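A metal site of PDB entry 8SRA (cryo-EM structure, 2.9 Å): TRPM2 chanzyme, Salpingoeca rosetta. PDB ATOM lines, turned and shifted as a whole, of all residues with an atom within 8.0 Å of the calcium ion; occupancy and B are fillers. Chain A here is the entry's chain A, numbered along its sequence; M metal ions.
O of Trp 620 touches the calcium ion (3.7 Å).
Ser 626 touches the calcium ion.
Of the 19 residues printed, 5 come within 4 Å of the calcium ion.
OG1 of Thr 1117 is in hydrogen-bond range of OG of Ser 626 (3.4 Å).
OG of Ser 600 lies within hydrogen-bond range of N of Gly 623 (3.4 Å).
N of Ser 626 sits at hydrogen-bond distance from OE2 of Glu 1113 (3.2 Å).
NE1 of Trp 620 is in hydrogen-bond range of O of Ser 626.
The side-chain hydroxyl (OG) of Ser 626 lies close to the side-chain carboxylate (OE2) of Glu 1114 (3.2 Å).
The calcium ion is bound by the backbone carbonyl oxygen (O) of Leu 621 (2.1 Å).
The calcium ion is bound by the side-chain carboxylate (OE2) of Glu 1114 (2.4 Å).
The calcium ion is bound by OE1 of Glu 1114, at 2.5 Å.
The backbone carbonyl oxygen (O) of Gly 623 is bound to the calcium ion, at 2.5 Å.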
ATOM      1  N   PHE A 593      19.393  19.990  33.989  1.00  0.00           N
ATOM      2  CA  PHE A 593      20.288  20.472  32.906  1.00  0.00           C
ATOM      3  C   PHE A 593      21.014  21.735  33.375  1.00  0.00           C
ATOM      4  O   PHE A 593      22.211  21.839  33.140  1.00  0.00           O
ATOM      5  CB  PHE A 593      19.496  20.846  31.658  1.00  0.00           C
ATOM      6  CG  PHE A 593      20.352  21.195  30.469  1.00  0.00           C
ATOM      7  CD1 PHE A 593      21.449  20.423  30.141  1.00  0.00           C
ATOM      8  CD2 PHE A 593      20.054  22.299  29.685  1.00  0.00           C
ATOM      9  CE1 PHE A 593      22.232  20.740  29.048  1.00  0.00           C
ATOM     10  CE2 PHE A 593      20.844  22.614  28.586  1.00  0.00           C
ATOM     11  CZ  PHE A 593      21.927  21.837  28.274  1.00  0.00           C
ATOM     12  N   SER A 600      29.428  21.766  34.939  1.00  0.00           N
ATOM     13  CA  SER A 600      30.213  21.541  33.727  1.00  0.00           C
ATOM     14  C   SER A 600      31.099  22.737  33.429  1.00  0.00           C
ATOM     15  O   SER A 600      32.217  22.545  32.944  1.00  0.00           O
ATOM     16  CB  SER A 600      29.277  21.267  32.555  1.00  0.00           C
ATOM     17  OG  SER A 600      30.016  21.145  31.366  1.00  0.00           O
ATOM     18  N   ARG A 617      37.154  19.853  26.198  1.00  0.00           N
ATOM     19  CA  ARG A 617      36.260  19.628  25.079  1.00  0.00           C
ATOM     20  C   ARG A 617      35.024  18.846  25.530  1.00  0.00           C
ATOM     21  O   ARG A 617      33.907  19.149  25.093  1.00  0.00           O
ATOM     22  CB  ARG A 617      37.008  18.885  23.975  1.00  0.00           C
ATOM     23  CG  ARG A 617      36.233  18.656  22.715  1.00  0.00           C
ATOM     24  CD  ARG A 617      36.906  17.594  21.902  1.00  0.00           C
ATOM     25  NE  ARG A 617      36.473  17.578  20.516  1.00  0.00           N
ATOM     26  CZ  ARG A 617      35.428  16.884  20.079  1.00  0.00           C
ATOM     27  NH1 ARG A 617      34.701  16.147  20.892  1.00  0.00           N
ATOM     28  NH2 ARG A 617      35.137  16.913  18.786  1.00  0.00           N
ATOM     29  N   HIS A 618      35.239  17.870  26.433  1.00  0.00           N
ATOM     30  CA  HIS A 618      34.145  17.077  26.998  1.00  0.00           C
ATOM     31  C   HIS A 618      33.194  17.877  27.886  1.00  0.00           C
ATOM     32  O   HIS A 618      31.968  17.746  27.759  1.00  0.00           O
ATOM     33  CB  HIS A 618      34.710  15.883  27.740  1.00  0.00           C
ATOM     34  CG  HIS A 618      33.663  14.992  28.310  1.00  0.00           C
ATOM     35  ND1 HIS A 618      32.819  14.230  27.532  1.00  0.00           N
ATOM     36  CD2 HIS A 618      33.374  14.684  29.592  1.00  0.00           C
ATOM     37  CE1 HIS A 618      31.993  13.572  28.325  1.00  0.00           C
ATOM     38  NE2 HIS A 618      32.345  13.772  29.571  1.00  0.00           N
ATOM     39  N   PHE A 619      33.727  18.704  28.800  1.00  0.00           N
ATOM     40  CA  PHE A 619      32.888  19.555  29.651  1.00  0.00           C
ATOM     41  C   PHE A 619      32.253  20.697  28.872  1.00  0.00           C
ATOM     42  O   PHE A 619      31.213  21.207  29.299  1.00  0.00           O
ATOM     43  CB  PHE A 619      33.625  20.079  30.876  1.00  0.00           C
ATOM     44  CG  PHE A 619      34.015  19.008  31.852  1.00  0.00           C
ATOM     45  CD1 PHE A 619      33.061  18.083  32.266  1.00  0.00           C
ATOM     46  CD2 PHE A 619      35.289  19.010  32.440  1.00  0.00           C
ATOM     47  CE1 PHE A 619      33.388  17.092  33.197  1.00  0.00           C
ATOM     48  CE2 PHE A 619      35.637  18.015  33.364  1.00  0.00           C
ATOM     49  CZ  PHE A 619      34.674  17.073  33.747  1.00  0.00           C
ATOM     50  N   TRP A 620      32.927  21.180  27.819  1.00  0.00           N
ATOM     51  CA  TRP A 620      32.351  22.162  26.907  1.00  0.00           C
ATOM     52  C   TRP A 620      31.170  21.565  26.149  1.00  0.00           C
ATOM     53  O   TRP A 620      30.163  22.253  25.919  1.00  0.00           O
ATOM     54  CB  TRP A 620      33.417  22.643  25.949  1.00  0.00           C
ATOM     55  CG  TRP A 620      32.931  23.441  24.813  1.00  0.00           C
ATOM     56  CD1 TRP A 620      32.595  24.749  24.826  1.00  0.00           C
ATOM     57  CD2 TRP A 620      32.778  23.000  23.467  1.00  0.00           C
ATOM     58  NE1 TRP A 620      32.206  25.162  23.583  1.00  0.00           N
ATOM     59  CE2 TRP A 620      32.309  24.101  22.720  1.00  0.00           C
ATOM     60  CE3 TRP A 620      32.966  21.780  22.809  1.00  0.00           C
ATOM     61  CZ2 TRP A 620      32.040  24.019  21.357  1.00  0.00           C
ATOM     62  CZ3 TRP A 620      32.696  21.689  21.448  1.00  0.00           C
ATOM     63  CH2 TRP A 620      32.231  22.818  20.738  1.00  0.00           C
ATOM     64  N   LEU A 621      31.256  20.287  25.827  1.00  0.00           N
ATOM     65  CA  LEU A 621      30.159  19.678  25.054  1.00  0.00           C
ATOM     66  C   LEU A 621      28.997  19.424  26.016  1.00  0.00           C
ATOM     67  O   LEU A 621      27.854  19.746  25.648  1.00  0.00           O
ATOM     68  CB  LEU A 621      30.652  18.386  24.414  1.00  0.00           C
ATOM     69  CG  LEU A 621      29.731  17.788  23.364  1.00  0.00           C
ATOM     70  CD1 LEU A 621      29.324  18.842  22.350  1.00  0.00           C
ATOM     71  CD2 LEU A 621      30.407  16.617  22.662  1.00  0.00           C
ATOM     72  N   ILE A 622      29.296  18.916  27.204  1.00  0.00           N
ATOM     73  CA  ILE A 622      28.213  18.602  28.162  1.00  0.00           C
ATOM     74  C   ILE A 622      27.329  19.816  28.450  1.00  0.00           C
ATOM     75  O   ILE A 622      26.102  19.733  28.348  1.00  0.00           O
ATOM     76  CB  ILE A 622      28.795  17.997  29.469  1.00  0.00           C
ATOM     77  CG1 ILE A 622      29.204  16.548  29.230  1.00  0.00           C
ATOM     78  CG2 ILE A 622      27.870  18.167  30.735  1.00  0.00           C
ATOM     79  CD1 ILE A 622      29.730  15.835  30.447  1.00  0.00           C
ATOM     80  N   GLY A 623      27.940  20.967  28.687  1.00  0.00           N
ATOM     81  CA  GLY A 623      27.197  22.164  29.016  1.00  0.00           C
ATOM     82  C   GLY A 623      26.561  22.841  27.818  1.00  0.00           C
ATOM     83  O   GLY A 623      26.518  22.336  26.699  1.00  0.00           O
ATOM     84  N   ASP A 624      26.066  24.036  28.073  1.00  0.00           N
ATOM     85  CA  ASP A 624      25.429  24.812  27.042  1.00  0.00           C
ATOM     86  C   ASP A 624      26.286  26.051  26.873  1.00  0.00           C
ATOM     87  O   ASP A 624      27.343  26.132  27.525  1.00  0.00           O
ATOM     88  CB  ASP A 624      23.973  25.110  27.423  1.00  0.00           C
ATOM     89  CG  ASP A 624      23.851  26.163  28.514  1.00  0.00           C
ATOM     90  OD1 ASP A 624      24.511  26.035  29.553  1.00  0.00           O
ATOM     91  OD2 ASP A 624      23.073  27.112  28.319  1.00  0.00           O
ATOM     92  N   GLN A 625      25.803  26.976  26.028  1.00  0.00           N
ATOM     93  CA  GLN A 625      26.391  28.254  25.629  1.00  0.00           C
ATOM     94  C   GLN A 625      27.788  28.019  25.041  1.00  0.00           C
ATOM     95  O   GLN A 625      28.776  28.518  25.545  1.00  0.00           O
ATOM     96  CB  GLN A 625      26.427  29.254  26.791  1.00  0.00           C
ATOM     97  CG  GLN A 625      25.073  29.825  27.108  1.00  0.00           C
ATOM     98  CD  GLN A 625      24.472  30.620  25.992  1.00  0.00           C
ATOM     99  OE1 GLN A 625      24.939  31.699  25.656  1.00  0.00           O
ATOM    100  NE2 GLN A 625      23.409  30.097  25.394  1.00  0.00           N
ATOM    101  N   SER A 626      27.797  27.156  24.007  1.00  0.00           N
ATOM    102  CA  SER A 626      28.995  26.549  23.407  1.00  0.00           C
ATOM    103  C   SER A 626      29.934  27.561  22.778  1.00  0.00           C
ATOM    104  O   SER A 626      31.167  27.438  22.925  1.00  0.00           O
ATOM    105  CB  SER A 626      28.565  25.516  22.361  1.00  0.00           C
ATOM    106  OG  SER A 626      27.742  24.530  22.936  1.00  0.00           O
ATOM    107  N   THR A1110      18.784  27.778  23.219  1.00  0.00           N
ATOM    108  CA  THR A1110      19.660  26.774  23.857  1.00  0.00           C
ATOM    109  C   THR A1110      19.618  25.420  23.136  1.00  0.00           C
ATOM    110  O   THR A1110      20.674  24.846  22.846  1.00  0.00           O
ATOM    111  CB  THR A1110      19.239  26.654  25.320  1.00  0.00           C
ATOM    112  OG1 THR A1110      19.502  27.897  25.978  1.00  0.00           O
ATOM    113  CG2 THR A1110      20.016  25.580  26.057  1.00  0.00           C
ATOM    114  N   GLU A1113      21.220  25.766  19.593  1.00  0.00           N
ATOM    115  CA  GLU A1113      22.672  25.883  19.729  1.00  0.00           C
ATOM    116  C   GLU A1113      23.335  24.538  20.030  1.00  0.00           C
ATOM    117  O   GLU A1113      24.390  24.239  19.447  1.00  0.00           O
ATOM    118  CB  GLU A1113      22.979  26.892  20.835  1.00  0.00           C
ATOM    119  CG  GLU A1113      24.436  27.155  21.113  1.00  0.00           C
ATOM    120  CD  GLU A1113      24.633  28.274  22.105  1.00  0.00           C
ATOM    121  OE1 GLU A1113      23.662  28.612  22.813  1.00  0.00           O
ATOM    122  OE2 GLU A1113      25.749  28.825  22.172  1.00  0.00           O
ATOM    123  N   GLU A1114      22.713  23.723  20.915  1.00  0.00           N
ATOM    124  CA  GLU A1114      23.228  22.389  21.240  1.00  0.00           C
ATOM    125  C   GLU A1114      23.140  21.431  20.057  1.00  0.00           C
ATOM    126  O   GLU A1114      24.080  20.649  19.838  1.00  0.00           O
ATOM    127  CB  GLU A1114      22.515  21.791  22.450  1.00  0.00           C
ATOM    128  CG  GLU A1114      22.857  22.461  23.760  1.00  0.00           C
ATOM    129  CD  GLU A1114      24.247  22.111  24.263  1.00  0.00           C
ATOM    130  OE1 GLU A1114      24.431  21.029  24.857  1.00  0.00           O
ATOM    131  OE2 GLU A1114      25.156  22.933  24.054  1.00  0.00           O
ATOM    132  N   LEU A1115      22.046  21.538  19.307  1.00  0.00           N
ATOM    133  CA  LEU A1115      21.860  20.655  18.132  1.00  0.00           C
ATOM    134  C   LEU A1115      22.932  21.000  17.124  1.00  0.00           C
ATOM    135  O   LEU A1115      23.650  20.101  16.686  1.00  0.00           O
ATOM    136  CB  LEU A1115      20.489  20.938  17.527  1.00  0.00           C
ATOM    137  CG  LEU A1115      20.150  20.164  16.255  1.00  0.00           C
ATOM    138  CD1 LEU A1115      20.120  18.673  16.534  1.00  0.00           C
ATOM    139  CD2 LEU A1115      18.835  20.621  15.675  1.00  0.00           C
ATOM    140  N   THR A1117      25.739  22.426  17.506  1.00  0.00           N
ATOM    141  CA  THR A1117      27.046  22.031  18.044  1.00  0.00           C
ATOM    142  C   THR A1117      27.339  20.567  17.725  1.00  0.00           C
ATOM    143  O   THR A1117      28.456  20.245  17.254  1.00  0.00           O
ATOM    144  CB  THR A1117      27.079  22.275  19.554  1.00  0.00           C
ATOM    145  OG1 THR A1117      26.709  23.623  19.821  1.00  0.00           O
ATOM    146  CG2 THR A1117      28.448  22.036  20.127  1.00  0.00           C
ATOM    147  N   ASP A1118      26.332  19.696  17.942  1.00  0.00           N
ATOM    148  CA  ASP A1118      26.421  18.259  17.603  1.00  0.00           C
ATOM    149  C   ASP A1118      26.581  18.028  16.105  1.00  0.00           C
ATOM    150  O   ASP A1118      27.359  17.151  15.704  1.00  0.00           O
ATOM    151  CB  ASP A1118      25.221  17.477  18.119  1.00  0.00           C
ATOM    152  CG  ASP A1118      25.067  17.572  19.611  1.00  0.00           C
ATOM    153  OD1 ASP A1118      26.075  17.405  20.327  1.00  0.00           O
ATOM    154  OD2 ASP A1118      23.912  17.692  20.085  1.00  0.00           O
ATOM    155  N   LEU A1121      30.161  18.970  14.992  1.00  0.00           N
ATOM    156  CA  LEU A1121      31.102  17.924  15.434  1.00  0.00           C
ATOM    157  C   LEU A1121      31.041  16.673  14.560  1.00  0.00           C
ATOM    158  O   LEU A1121      32.094  16.073  14.290  1.00  0.00           O
ATOM    159  CB  LEU A1121      30.884  17.589  16.907  1.00  0.00           C
ATOM    160  CG  LEU A1121      31.364  18.638  17.911  1.00  0.00           C
ATOM    161  CD1 LEU A1121      31.284  18.084  19.305  1.00  0.00           C
ATOM    162  CD2 LEU A1121      32.761  19.185  17.636  1.00  0.00           C
HETATM  163 CA    CA M   1      26.854  21.228  24.504  1.00  0.00          CA
